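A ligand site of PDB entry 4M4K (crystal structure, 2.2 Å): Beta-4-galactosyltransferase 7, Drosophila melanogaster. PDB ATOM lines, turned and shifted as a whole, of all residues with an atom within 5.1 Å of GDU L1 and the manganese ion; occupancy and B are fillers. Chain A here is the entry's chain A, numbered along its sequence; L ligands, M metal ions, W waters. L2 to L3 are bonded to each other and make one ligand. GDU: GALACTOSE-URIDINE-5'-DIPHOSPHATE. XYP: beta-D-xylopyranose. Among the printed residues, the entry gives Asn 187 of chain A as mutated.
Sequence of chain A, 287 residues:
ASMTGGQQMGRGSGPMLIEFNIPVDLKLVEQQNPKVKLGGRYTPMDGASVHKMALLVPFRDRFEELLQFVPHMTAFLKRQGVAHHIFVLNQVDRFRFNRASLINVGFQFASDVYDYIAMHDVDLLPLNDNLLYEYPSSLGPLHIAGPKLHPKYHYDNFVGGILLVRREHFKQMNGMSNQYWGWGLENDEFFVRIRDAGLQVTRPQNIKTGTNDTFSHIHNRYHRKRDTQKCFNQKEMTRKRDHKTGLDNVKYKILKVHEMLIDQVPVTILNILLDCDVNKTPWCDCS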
ATOM      1  N   VAL A  57       8.502 -17.777  14.950  1.00  0.00           N
ATOM      2  CA  VAL A  57       9.500 -18.817  14.765  1.00  0.00           C
ATOM      3  C   VAL A  57      10.555 -18.778  15.856  1.00  0.00           C
ATOM      4  O   VAL A  57      11.566 -18.085  15.732  1.00  0.00           O
ATOM      5  CB  VAL A  57      10.224 -18.651  13.438  1.00  0.00           C
ATOM      6  CG1 VAL A  57      11.158 -19.835  13.202  1.00  0.00           C
ATOM      7  CG2 VAL A  57       9.203 -18.551  12.298  1.00  0.00           C
ATOM      8  N   PRO A  58      10.305 -19.512  16.945  1.00  0.00           N
ATOM      9  CA  PRO A  58      11.328 -19.683  17.992  1.00  0.00           C
ATOM     10  C   PRO A  58      12.596 -20.163  17.326  1.00  0.00           C
ATOM     11  O   PRO A  58      12.547 -21.060  16.489  1.00  0.00           O
ATOM     12  CB  PRO A  58      10.761 -20.814  18.851  1.00  0.00           C
ATOM     13  CG  PRO A  58       9.276 -20.740  18.646  1.00  0.00           C
ATOM     14  CD  PRO A  58       9.080 -20.271  17.216  1.00  0.00           C
ATOM     15  N   PHE A  59      13.732 -19.556  17.677  1.00  0.00           N
ATOM     16  CA  PHE A  59      14.908 -19.724  16.869  1.00  0.00           C
ATOM     17  C   PHE A  59      16.197 -19.636  17.677  1.00  0.00           C
ATOM     18  O   PHE A  59      16.354 -18.731  18.508  1.00  0.00           O
ATOM     19  CB  PHE A  59      14.898 -18.633  15.800  1.00  0.00           C
ATOM     20  CG  PHE A  59      16.006 -18.747  14.804  1.00  0.00           C
ATOM     21  CD1 PHE A  59      15.837 -19.501  13.655  1.00  0.00           C
ATOM     22  CD2 PHE A  59      17.216 -18.106  15.002  1.00  0.00           C
ATOM     23  CE1 PHE A  59      16.856 -19.614  12.716  1.00  0.00           C
ATOM     24  CE2 PHE A  59      18.228 -18.206  14.087  1.00  0.00           C
ATOM     25  CZ  PHE A  59      18.058 -18.957  12.928  1.00  0.00           C
ATOM     26  N   ARG A  60      17.099 -20.588  17.444  1.00  0.00           N
ATOM     27  CA  ARG A  60      18.505 -20.410  17.821  1.00  0.00           C
ATOM     28  C   ARG A  60      19.373 -21.299  16.949  1.00  0.00           C
ATOM     29  O   ARG A  60      19.154 -22.507  16.874  1.00  0.00           O
ATOM     30  CB  ARG A  60      18.751 -20.728  19.294  1.00  0.00           C
ATOM     31  CG  ARG A  60      20.254 -20.681  19.662  1.00  0.00           C
ATOM     32  CD  ARG A  60      20.507 -21.336  20.984  1.00  0.00           C
ATOM     33  NE  ARG A  60      20.208 -20.436  22.081  1.00  0.00           N
ATOM     34  CZ  ARG A  60      19.914 -20.827  23.316  1.00  0.00           C
ATOM     35  NH1 ARG A  60      19.847 -22.130  23.610  1.00  0.00           N
ATOM     36  NH2 ARG A  60      19.680 -19.919  24.257  1.00  0.00           N
ATOM     37  N   ARG A  62      19.838 -21.864  13.680  1.00  0.00           N
ATOM     38  CA  ARG A  62      19.208 -22.654  12.619  1.00  0.00           C
ATOM     39  C   ARG A  62      19.185 -21.810  11.355  1.00  0.00           C
ATOM     40  O   ARG A  62      18.156 -21.657  10.693  1.00  0.00           O
ATOM     41  CB  ARG A  62      17.788 -23.079  13.003  1.00  0.00           C
ATOM     42  CG  ARG A  62      17.705 -23.956  14.239  1.00  0.00           C
ATOM     43  CD  ARG A  62      18.374 -25.303  14.014  1.00  0.00           C
ATOM     44  NE  ARG A  62      18.213 -26.200  15.160  1.00  0.00           N
ATOM     45  CZ  ARG A  62      19.129 -26.378  16.110  1.00  0.00           C
ATOM     46  NH1 ARG A  62      20.284 -25.731  16.049  1.00  0.00           N
ATOM     47  NH2 ARG A  62      18.890 -27.224  17.108  1.00  0.00           N
ATOM     48  N   PHE A  97      17.292 -24.061  25.225  1.00  0.00           N
ATOM     49  CA  PHE A  97      16.276 -23.536  24.333  1.00  0.00           C
ATOM     50  C   PHE A  97      14.874 -23.609  24.910  1.00  0.00           C
ATOM     51  O   PHE A  97      14.395 -24.680  25.306  1.00  0.00           O
ATOM     52  CB  PHE A  97      16.338 -24.235  22.973  1.00  0.00           C
ATOM     53  CG  PHE A  97      15.531 -23.564  21.918  1.00  0.00           C
ATOM     54  CD1 PHE A  97      15.947 -22.358  21.378  1.00  0.00           C
ATOM     55  CD2 PHE A  97      14.344 -24.130  21.467  1.00  0.00           C
ATOM     56  CE1 PHE A  97      15.193 -21.730  20.383  1.00  0.00           C
ATOM     57  CE2 PHE A  97      13.595 -23.513  20.480  1.00  0.00           C
ATOM     58  CZ  PHE A  97      14.020 -22.302  19.940  1.00  0.00           C
ATOM     59  N   ARG A  99      11.375 -22.846  23.711  1.00  0.00           N
ATOM     60  CA  ARG A  99      10.480 -22.546  22.607  1.00  0.00           C
ATOM     61  C   ARG A  99       9.230 -21.798  23.064  1.00  0.00           C
ATOM     62  O   ARG A  99       8.820 -20.786  22.478  1.00  0.00           O
ATOM     63  CB  ARG A  99      10.081 -23.874  21.943  1.00  0.00           C
ATOM     64  CG  ARG A  99       9.118 -23.732  20.796  1.00  0.00           C
ATOM     65  CD  ARG A  99       8.412 -25.053  20.472  1.00  0.00           C
ATOM     66  NE  ARG A  99       7.599 -24.876  19.279  1.00  0.00           N
ATOM     67  CZ  ARG A  99       6.326 -25.225  19.157  1.00  0.00           C
ATOM     68  NH1 ARG A  99       5.664 -25.790  20.164  1.00  0.00           N
ATOM     69  NH2 ARG A  99       5.709 -24.994  18.001  1.00  0.00           N
ATOM     70  N   HIS A 120       5.523 -21.837  14.825  1.00  0.00           N
ATOM     71  CA  HIS A 120       6.017 -22.586  13.670  1.00  0.00           C
ATOM     72  C   HIS A 120       7.476 -23.046  13.819  1.00  0.00           C
ATOM     73  O   HIS A 120       8.364 -22.218  13.951  1.00  0.00           O
ATOM     74  CB  HIS A 120       5.938 -21.695  12.428  1.00  0.00           C
ATOM     75  CG  HIS A 120       5.630 -22.433  11.159  1.00  0.00           C
ATOM     76  ND1 HIS A 120       6.431 -23.448  10.677  1.00  0.00           N
ATOM     77  CD2 HIS A 120       4.610 -22.296  10.280  1.00  0.00           C
ATOM     78  CE1 HIS A 120       5.912 -23.910   9.544  1.00  0.00           C
ATOM     79  NE2 HIS A 120       4.801 -23.226   9.287  1.00  0.00           N
ATOM     80  N   ASP A 121       7.715 -24.356  13.773  1.00  0.00           N
ATOM     81  CA  ASP A 121       9.074 -24.855  13.668  1.00  0.00           C
ATOM     82  C   ASP A 121       9.751 -24.361  12.393  1.00  0.00           C
ATOM     83  O   ASP A 121       9.109 -24.268  11.346  1.00  0.00           O
ATOM     84  CB  ASP A 121       9.091 -26.375  13.683  1.00  0.00           C
ATOM     85  CG  ASP A 121       8.544 -26.954  14.965  1.00  0.00           C
ATOM     86  OD1 ASP A 121       8.232 -26.187  15.917  1.00  0.00           O
ATOM     87  OD2 ASP A 121       8.437 -28.193  15.028  1.00  0.00           O
ATOM     88  N   VAL A 122      11.042 -24.048  12.456  1.00  0.00           N
ATOM     89  CA  VAL A 122      11.752 -23.465  11.316  1.00  0.00           C
ATOM     90  C   VAL A 122      12.093 -24.522  10.250  1.00  0.00           C
ATOM     91  O   VAL A 122      12.397 -24.179   9.107  1.00  0.00           O
ATOM     92  CB  VAL A 122      13.032 -22.745  11.779  1.00  0.00           C
ATOM     93  CG1 VAL A 122      14.118 -23.772  12.109  1.00  0.00           C
ATOM     94  CG2 VAL A 122      13.533 -21.751  10.727  1.00  0.00           C
ATOM     95  N   ASP A 123      12.026 -25.806  10.618  1.00  0.00           N
ATOM     96  CA  ASP A 123      12.495 -26.904   9.769  1.00  0.00           C
ATOM     97  C   ASP A 123      11.339 -27.719   9.180  1.00  0.00           C
ATOM     98  O   ASP A 123      11.542 -28.801   8.618  1.00  0.00           O
ATOM     99  CB  ASP A 123      13.392 -27.850  10.566  1.00  0.00           C
ATOM    100  CG  ASP A 123      12.677 -28.449  11.774  1.00  0.00           C
ATOM    101  OD1 ASP A 123      11.464 -28.188  11.949  1.00  0.00           O
ATOM    102  OD2 ASP A 123      13.333 -29.191  12.552  1.00  0.00           O
ATOM    103  N   LEU A 124      10.128 -27.205   9.338  1.00  0.00           N
ATOM    104  CA  LEU A 124       8.918 -27.959   8.977  1.00  0.00           C
ATOM    105  C   LEU A 124       8.108 -27.189   7.930  1.00  0.00           C
ATOM    106  O   LEU A 124       7.531 -26.129   8.230  1.00  0.00           O
ATOM    107  CB  LEU A 124       8.099 -28.246  10.238  1.00  0.00           C
ATOM    108  CG  LEU A 124       6.989 -29.308  10.172  1.00  0.00           C
ATOM    109  CD1 LEU A 124       7.575 -30.664   9.798  1.00  0.00           C
ATOM    110  CD2 LEU A 124       6.263 -29.378  11.525  1.00  0.00           C
ATOM    111  N   HIS A 150       1.967 -35.586  10.018  1.00  0.00           N
ATOM    112  CA  HIS A 150       3.354 -35.345  10.428  1.00  0.00           C
ATOM    113  C   HIS A 150       4.221 -36.597  10.205  1.00  0.00           C
ATOM    114  O   HIS A 150       3.798 -37.714  10.517  1.00  0.00           O
ATOM    115  CB  HIS A 150       3.409 -34.893  11.888  1.00  0.00           C
ATOM    116  CG  HIS A 150       4.709 -34.285  12.288  1.00  0.00           C
ATOM    117  ND1 HIS A 150       5.831 -35.037  12.573  1.00  0.00           N
ATOM    118  CD2 HIS A 150       5.087 -32.992  12.428  1.00  0.00           C
ATOM    119  CE1 HIS A 150       6.834 -34.246  12.874  1.00  0.00           C
ATOM    120  NE2 HIS A 150       6.410 -32.986  12.791  1.00  0.00           N
ATOM    121  N   TYR A 153       5.588 -37.566  14.363  1.00  0.00           N
ATOM    122  CA  TYR A 153       4.768 -37.596  15.578  1.00  0.00           C
ATOM    123  C   TYR A 153       3.325 -37.886  15.275  1.00  0.00           C
ATOM    124  O   TYR A 153       2.673 -37.129  14.540  1.00  0.00           O
ATOM    125  CB  TYR A 153       4.909 -36.264  16.332  1.00  0.00           C
ATOM    126  CG  TYR A 153       6.346 -35.963  16.678  1.00  0.00           C
ATOM    127  CD1 TYR A 153       7.090 -36.843  17.457  1.00  0.00           C
ATOM    128  CD2 TYR A 153       6.954 -34.790  16.251  1.00  0.00           C
ATOM    129  CE1 TYR A 153       8.410 -36.574  17.795  1.00  0.00           C
ATOM    130  CE2 TYR A 153       8.268 -34.508  16.572  1.00  0.00           C
ATOM    131  CZ  TYR A 153       8.985 -35.401  17.350  1.00  0.00           C
ATOM    132  OH  TYR A 153      10.289 -35.123  17.661  1.00  0.00           O
ATOM    133  N   PHE A 158      -1.022 -34.722  19.703  1.00  0.00           N
ATOM    134  CA  PHE A 158       0.144 -33.974  19.241  1.00  0.00           C
ATOM    135  C   PHE A 158      -0.345 -32.657  18.634  1.00  0.00           C
ATOM    136  O   PHE A 158      -1.150 -32.667  17.703  1.00  0.00           O
ATOM    137  CB  PHE A 158       0.947 -34.770  18.207  1.00  0.00           C
ATOM    138  CG  PHE A 158       2.012 -33.966  17.519  1.00  0.00           C
ATOM    139  CD1 PHE A 158       3.182 -33.602  18.191  1.00  0.00           C
ATOM    140  CD2 PHE A 158       1.863 -33.576  16.194  1.00  0.00           C
ATOM    141  CE1 PHE A 158       4.174 -32.856  17.558  1.00  0.00           C
ATOM    142  CE2 PHE A 158       2.850 -32.841  15.549  1.00  0.00           C
ATOM    143  CZ  PHE A 158       4.008 -32.475  16.232  1.00  0.00           C
ATOM    144  N   GLY A 160       2.181 -30.162  18.128  1.00  0.00           N
ATOM    145  CA  GLY A 160       3.443 -29.502  17.878  1.00  0.00           C
ATOM    146  C   GLY A 160       3.644 -29.099  16.428  1.00  0.00           C
ATOM    147  O   GLY A 160       2.729 -29.227  15.596  1.00  0.00           O
ATOM    148  N   GLY A 161       4.832 -28.586  16.116  1.00  0.00           N
ATOM    149  CA  GLY A 161       5.196 -28.269  14.751  1.00  0.00           C
ATOM    150  C   GLY A 161       4.578 -26.987  14.228  1.00  0.00           C
ATOM    151  O   GLY A 161       5.272 -25.977  14.071  1.00  0.00           O
ATOM    152  N   GLY A 182      14.754 -26.663  27.271  1.00  0.00           N
ATOM    153  CA  GLY A 182      15.206 -27.845  26.571  1.00  0.00           C
ATOM    154  C   GLY A 182      14.037 -28.513  25.846  1.00  0.00           C
ATOM    155  O   GLY A 182      12.877 -28.131  26.048  1.00  0.00           O
ATOM    156  N   TRP A 183      14.348 -29.514  25.036  1.00  0.00           N
ATOM    157  CA  TRP A 183      13.372 -30.164  24.187  1.00  0.00           C
ATOM    158  C   TRP A 183      12.202 -30.797  24.944  1.00  0.00           C
ATOM    159  O   TRP A 183      12.383 -31.410  26.014  1.00  0.00           O
ATOM    160  CB  TRP A 183      14.062 -31.239  23.357  1.00  0.00           C
ATOM    161  CG  TRP A 183      13.139 -31.974  22.388  1.00  0.00           C
ATOM    162  CD1 TRP A 183      12.936 -31.678  21.060  1.00  0.00           C
ATOM    163  CD2 TRP A 183      12.323 -33.125  22.661  1.00  0.00           C
ATOM    164  NE1 TRP A 183      12.047 -32.563  20.500  1.00  0.00           N
ATOM    165  CE2 TRP A 183      11.656 -33.462  21.459  1.00  0.00           C
ATOM    166  CE3 TRP A 183      12.091 -33.898  23.814  1.00  0.00           C
ATOM    167  CZ2 TRP A 183      10.765 -34.541  21.384  1.00  0.00           C
ATOM    168  CZ3 TRP A 183      11.213 -34.979  23.727  1.00  0.00           C
ATOM    169  CH2 TRP A 183      10.554 -35.289  22.519  1.00  0.00           C
ATOM    170  N   GLY A 184      10.997 -30.626  24.390  1.00  0.00           N
ATOM    171  CA  GLY A 184       9.886 -31.488  24.715  1.00  0.00           C
ATOM    172  C   GLY A 184       8.853 -30.997  25.702  1.00  0.00           C
ATOM    173  O   GLY A 184       9.145 -30.146  26.564  1.00  0.00           O
ATOM    174  N   LEU A 185       7.646 -31.553  25.538  1.00  0.00           N
ATOM    175  CA  LEU A 185       6.510 -31.424  26.458  1.00  0.00           C
ATOM    176  C   LEU A 185       5.754 -30.097  26.421  1.00  0.00           C
ATOM    177  O   LEU A 185       4.590 -30.060  26.808  1.00  0.00           O
ATOM    178  CB  LEU A 185       6.895 -31.780  27.894  1.00  0.00           C
ATOM    179  CG  LEU A 185       7.271 -33.244  28.138  1.00  0.00           C
ATOM    180  CD1 LEU A 185       7.731 -33.407  29.582  1.00  0.00           C
ATOM    181  CD2 LEU A 185       6.081 -34.179  27.825  1.00  0.00           C
ATOM    182  N   GLU A 186       6.375 -29.020  25.946  1.00  0.00           N
ATOM    183  CA  GLU A 186       5.730 -27.697  26.022  1.00  0.00           C
ATOM    184  C   GLU A 186       4.396 -27.671  25.269  1.00  0.00           C
ATOM    185  O   GLU A 186       3.407 -27.121  25.763  1.00  0.00           O
ATOM    186  CB  GLU A 186       6.688 -26.559  25.594  1.00  0.00           C
ATOM    187  CG  GLU A 186       6.728 -26.235  24.101  1.00  0.00           C
ATOM    188  CD  GLU A 186       7.253 -27.382  23.239  1.00  0.00           C
ATOM    189  OE1 GLU A 186       8.094 -28.179  23.740  1.00  0.00           O
ATOM    190  OE2 GLU A 186       6.824 -27.498  22.069  1.00  0.00           O
ATOM    191  N   ASN A 187       4.357 -28.301  24.101  1.00  0.00           N
ATOM    192  CA  ASN A 187       3.123 -28.390  23.320  1.00  0.00           C
ATOM    193  C   ASN A 187       2.075 -29.298  23.948  1.00  0.00           C
ATOM    194  O   ASN A 187       0.872 -29.072  23.780  1.00  0.00           O
ATOM    195  CB  ASN A 187       3.425 -28.894  21.906  1.00  0.00           C
ATOM    196  CG  ASN A 187       4.269 -30.148  21.898  1.00  0.00           C
ATOM    197  OD1 ASN A 187       5.210 -30.283  22.702  1.00  0.00           O
ATOM    198  ND2 ASN A 187       3.959 -31.077  20.993  1.00  0.00           N
ATOM    199  N   HIS A 217      10.377 -32.416   6.771  1.00  0.00           N
ATOM    200  CA  HIS A 217      11.005 -32.161   8.063  1.00  0.00           C
ATOM    201  C   HIS A 217      12.493 -32.417   7.900  1.00  0.00           C
ATOM    202  O   HIS A 217      12.998 -33.483   8.265  1.00  0.00           O
ATOM    203  CB  HIS A 217      10.442 -33.098   9.130  1.00  0.00           C
ATOM    204  CG  HIS A 217      10.943 -32.812  10.518  1.00  0.00           C
ATOM    205  ND1 HIS A 217      11.025 -33.772  11.503  1.00  0.00           N
ATOM    206  CD2 HIS A 217      11.396 -31.664  11.085  1.00  0.00           C
ATOM    207  CE1 HIS A 217      11.498 -33.236  12.612  1.00  0.00           C
ATOM    208  NE2 HIS A 217      11.741 -31.953  12.383  1.00  0.00           N
ATOM    209  N   HIS A 219      15.521 -32.362   9.237  1.00  0.00           N
ATOM    210  CA  HIS A 219      16.071 -32.317  10.590  1.00  0.00           C
ATOM    211  C   HIS A 219      16.840 -33.607  10.856  1.00  0.00           C
ATOM    212  O   HIS A 219      16.257 -34.625  11.248  1.00  0.00           O
ATOM    213  CB  HIS A 219      14.942 -32.161  11.616  1.00  0.00           C
ATOM    214  CG  HIS A 219      15.421 -31.970  13.030  1.00  0.00           C
ATOM    215  ND1 HIS A 219      14.612 -31.462  14.023  1.00  0.00           N
ATOM    216  CD2 HIS A 219      16.614 -32.231  13.610  1.00  0.00           C
ATOM    217  CE1 HIS A 219      15.284 -31.412  15.154  1.00  0.00           C
ATOM    218  NE2 HIS A 219      16.501 -31.865  14.935  1.00  0.00           N
ATOM    219  N   ARG A 226      18.595 -32.862  19.707  1.00  0.00           N
ATOM    220  CA  ARG A 226      17.532 -32.492  20.613  1.00  0.00           C
ATOM    221  C   ARG A 226      18.086 -32.459  22.035  1.00  0.00           C
ATOM    222  O   ARG A 226      18.673 -33.419  22.515  1.00  0.00           O
ATOM    223  CB  ARG A 226      16.352 -33.477  20.505  1.00  0.00           C
ATOM    224  CG  ARG A 226      15.658 -33.452  19.134  1.00  0.00           C
ATOM    225  CD  ARG A 226      14.484 -34.447  19.033  1.00  0.00           C
ATOM    226  NE  ARG A 226      13.710 -34.190  17.822  1.00  0.00           N
ATOM    227  CZ  ARG A 226      14.032 -34.625  16.602  1.00  0.00           C
ATOM    228  NH1 ARG A 226      15.105 -35.381  16.421  1.00  0.00           N
ATOM    229  NH2 ARG A 226      13.266 -34.318  15.551  1.00  0.00           N
HETATM  230  N1  GDU L   1      14.728 -24.698  17.602  1.00  0.00           N
HETATM  231  C2  GDU L   1      15.798 -23.895  17.412  1.00  0.00           C
HETATM  232  N3  GDU L   1      16.957 -24.108  18.013  1.00  0.00           N
HETATM  233  C4  GDU L   1      17.109 -25.142  18.868  1.00  0.00           C
HETATM  234  C5  GDU L   1      16.010 -26.004  19.111  1.00  0.00           C
HETATM  235  C6  GDU L   1      14.806 -25.739  18.431  1.00  0.00           C
HETATM  236  O2  GDU L   1      15.688 -22.950  16.650  1.00  0.00           O
HETATM  237  O4  GDU L   1      18.326 -25.385  19.521  1.00  0.00           O
HETATM  238  C1D GDU L   1      13.523 -24.411  16.977  1.00  0.00           C
HETATM  239  C2D GDU L   1      13.400 -24.790  15.503  1.00  0.00           C
HETATM  240  O2D GDU L   1      12.476 -23.887  14.956  1.00  0.00           O
HETATM  241  C3D GDU L   1      12.858 -26.140  15.579  1.00  0.00           C
HETATM  242  C4D GDU L   1      11.816 -25.956  16.614  1.00  0.00           C
HETATM  243  O4D GDU L   1      12.420 -25.112  17.625  1.00  0.00           O
HETATM  244  O3D GDU L   1      12.326 -26.596  14.336  1.00  0.00           O
HETATM  245  C5D GDU L   1      11.406 -27.270  17.246  1.00  0.00           C
HETATM  246  O5D GDU L   1      12.558 -27.885  17.756  1.00  0.00           O
HETATM  247  PA  GDU L   1      13.085 -29.272  17.127  1.00  0.00           P
HETATM  248  O1A GDU L   1      12.939 -29.277  15.589  1.00  0.00           O
HETATM  249  O2A GDU L   1      14.538 -29.422  17.504  1.00  0.00           O
HETATM  250  O3A GDU L   1      12.236 -30.502  17.755  1.00  0.00           O
HETATM  251  PB  GDU L   1      11.266 -31.493  16.979  1.00  0.00           P
HETATM  252  O1B GDU L   1      11.757 -31.740  15.525  1.00  0.00           O
HETATM  253  O2B GDU L   1      11.242 -32.806  17.736  1.00  0.00           O
HETATM  254  O3B GDU L   1       9.794 -30.845  16.925  1.00  0.00           O
HETATM  255  C1' GDU L   1       8.765 -31.175  17.858  1.00  0.00           C
HETATM  256  C2' GDU L   1       7.708 -30.211  17.677  1.00  0.00           C
HETATM  257  C3' GDU L   1       8.116 -28.922  18.171  1.00  0.00           C
HETATM  258  C4' GDU L   1       8.310 -28.945  19.629  1.00  0.00           C
HETATM  259  C5' GDU L   1       9.532 -29.888  20.025  1.00  0.00           C
HETATM  260  C6' GDU L   1       9.579 -30.160  21.368  1.00  0.00           C
HETATM  261  O2' GDU L   1       7.435 -30.113  16.167  1.00  0.00           O
HETATM  262  O3' GDU L   1       7.120 -27.872  17.777  1.00  0.00           O
HETATM  263  O4' GDU L   1       7.089 -29.421  20.224  1.00  0.00           O
HETATM  264  O5' GDU L   1       9.364 -31.208  19.213  1.00  0.00           O
HETATM  265  O6' GDU L   1      10.077 -29.155  22.019  1.00  0.00           O
HETATM  266  O1  XYP L   2       5.622 -41.842  23.124  1.00  0.00           O
HETATM  267  C1  XYP L   2       6.294 -40.609  23.253  1.00  0.00           C
HETATM  268  C2  XYP L   2       6.677 -40.122  21.875  1.00  0.00           C
HETATM  269  C3  XYP L   2       7.358 -38.813  21.986  1.00  0.00           C
HETATM  270  C4  XYP L   2       6.482 -37.832  22.620  1.00  0.00           C
HETATM  271  C5  XYP L   2       6.031 -38.291  23.977  1.00  0.00           C
HETATM  272  O2  XYP L   2       7.567 -41.088  21.253  1.00  0.00           O
HETATM  273  O3  XYP L   2       7.697 -38.308  20.687  1.00  0.00           O
HETATM  274  O4  XYP L   2       7.295 -36.638  22.772  1.00  0.00           O
HETATM  275  O5  XYP L   2       5.440 -39.651  23.942  1.00  0.00           O
HETATM  276  C1  XYP L   3       6.668 -35.567  22.161  1.00  0.00           C
HETATM  277  C2  XYP L   3       7.138 -34.295  22.871  1.00  0.00           C
HETATM  278  C3  XYP L   3       6.570 -33.114  22.195  1.00  0.00           C
HETATM  279  C4  XYP L   3       6.976 -33.071  20.778  1.00  0.00           C
HETATM  280  C5  XYP L   3       6.576 -34.372  20.038  1.00  0.00           C
HETATM  281  O2  XYP L   3       6.733 -34.363  24.253  1.00  0.00           O
HETATM  282  O3  XYP L   3       6.996 -31.912  22.875  1.00  0.00           O
HETATM  283  O4  XYP L   3       6.349 -31.973  20.091  1.00  0.00           O
HETATM  284  O5  XYP L   3       7.021 -35.574  20.750  1.00  0.00           O
HETATM  285 MN    MN M   1      12.462 -30.602  13.934  1.00  0.00          MN
HETATM  286  O   HOH W   1      10.376 -29.525  13.665  1.00  0.00           O
HETATM  287  O   HOH W   2      16.018 -27.878  15.542  1.00  0.00           O
HETATM  288  O   HOH W   3      12.131 -27.243  21.332  1.00  0.00           O
HETATM  289  O   HOH W   4      10.349 -27.244  24.922  1.00  0.00           O
HETATM  290  O   HOH W   5      14.261 -28.494  20.233  1.00  0.00           O
HETATM  291  O   HOH W   6       8.595 -31.626  13.942  1.00  0.00           O
HETATM  292  O   HOH W   7      17.311 -29.569  17.664  1.00  0.00           O
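An oxygen (O2) of GDU L1 is in hydrogen-bond range of the backbone NH of Arg 60 (2.9 Å). An oxygen (O3) of XYP L3 sits at hydrogen-bond distance from the backbone NH (N) of Leu 185 (2.8 Å). The side-chain amide oxygen of Asn 187 is in hydrogen-bond range of an oxygen (O4') of GDU L1, 3.2 Å away. An oxygen (O3') of GDU L1 is in hydrogen-bond range of the backbone NH of Gly 161 (2.9 Å). An oxygen (O2') of GDU L1 lies within hydrogen-bond range of the side-chain carboxylate (OD2) of Asp 121 (2.4 Å). The side-chain amide oxygen (OD1) of Asn 187 is in hydrogen-bond range of an oxygen (O3) of XYP L3, at 2.4 Å. The guanidinium group (NH2) of Arg 99 sits close to an oxygen (O3') of GDU L1 (3.2 Å). OE2 of Glu 186 lies within hydrogen-bond range of O4' of GDU L1 (2.7 Å). O2B of GDU L1 sits at hydrogen-bond distance from OH of Tyr 153 (2.5 Å). O of Pro 58 sits at hydrogen-bond distance from O2D of GDU L1 (3.2 Å). The guanidinium group (NE) of Arg 226 lies within salt-bridge range of an oxygen (O2B) of GDU L1 (2.8 Å). An oxygen (O2D) of GDU L1 lies within hydrogen-bond range of the backbone NH (N) of Val 122 (2.9 Å). An oxygen (O2B) of GDU L1 lies within hydrogen-bond range of the indole nitrogen (NE1) of Trp 183, at 2.9 Å. NH2 of Arg 62 is in hydrogen-bond range of O4 of GDU L1 (3.1 Å). The backbone carbonyl oxygen (O) of Arg 60 is in hydrogen-bond range of a nitrogen (N3) of GDU L1 (2.9 Å). N of Gly 184 is in hydrogen-bond range of O6' of GDU L1 (2.9 Å).
O4 of XYP L3 lies within hydrogen-bond range of O4' of GDU L1 (2.7 Å).
O of Phe 97 sits at hydrogen-bond distance from N of Gly 182, 2.8 Å away. The side-chain carboxylate (OE2) of Glu 186 is in salt-bridge range of the guanidinium group (NH1) of Arg 99, at 2.8 Å. N of Asp 121 sits at hydrogen-bond distance from O of Gly 161 (2.9 Å). OD1 of Asp 121 is in salt-bridge range of NH2 of Arg 99 (3.5 Å). The side-chain carboxylate (OE2) of Glu 186 lies close to the side-chain amide oxygen (OD1) of Asn 187, at 3.3 Å. A ring nitrogen (ND1) of His 150 is in hydrogen-bond range of the backbone NH of Tyr 153 (3.1 Å). The side-chain amide nitrogen (ND2) of Asn 187 lies close to the backbone NH (N) of Gly 160, at 3.5 Å.
Merely in contact with GDU L1: Phe 97 (3.3 Å), Phe 59 (3.3 Å) and Gly 160 (3.9 Å). Hydrophobic or aromatic side chains within 4 Å of GDU L1: Phe 97, Val 122, Tyr 153, Trp 183, His 217 and His 219. Within 4 Å of GDU L1: Pro 58, Phe 59, Arg 60, Arg 62, Phe 97, Arg 99, Asp 121, Val 122, Asp 123, Tyr 153, Gly 160, Gly 161, Trp 183, Gly 184, Glu 186, Asn 187, His 217, His 219 and Arg 226.
Three residues have an atom within 4 Å of the manganese ion: Asp 123, His 217 and His 219. The nearest printed residue that does not touch the manganese ion is Arg 226 (4.1 Å).
The manganese ion is bound by an oxygen (O1B) of GDU L1 (2.1 Å). The manganese ion is bound by the side-chain carboxylate (OD2) of Asp 123. O1A of GDU L1 is bound to the manganese ion. A ring nitrogen (NE2) of His 217 binds the manganese ion (2.2 Å). ND1 of His 219 is bound to the manganese ion, 2.3 Å away. The manganese ion is bound by water W1.
Water W1 bridges the side-chain carboxylate (OD1) of Asp 123 (2.4 Å) and the side-chain carboxylate (OD2) of Asp 121 (2.7 Å). Water W7 lies within hydrogen-bond range of an oxygen (O2A) of GDU L1 (2.8 Å) and the guanidinium group of Arg 62 (2.9 Å). Water W2 bridges the guanidinium group (NE) of Arg 62 (2.8 Å) and an oxygen (O2A) of GDU L1 (2.9 Å). Water W6 lies within hydrogen-bond range of NE2 of His 150 and O2' of GDU L1. Water W4 lies within hydrogen-bond range of the side-chain carboxylate (OE1) of Glu 186, the backbone carbonyl oxygen (O) of Gly 182, the backbone NH (N) of Gly 184 and an oxygen (O6') of GDU L1.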
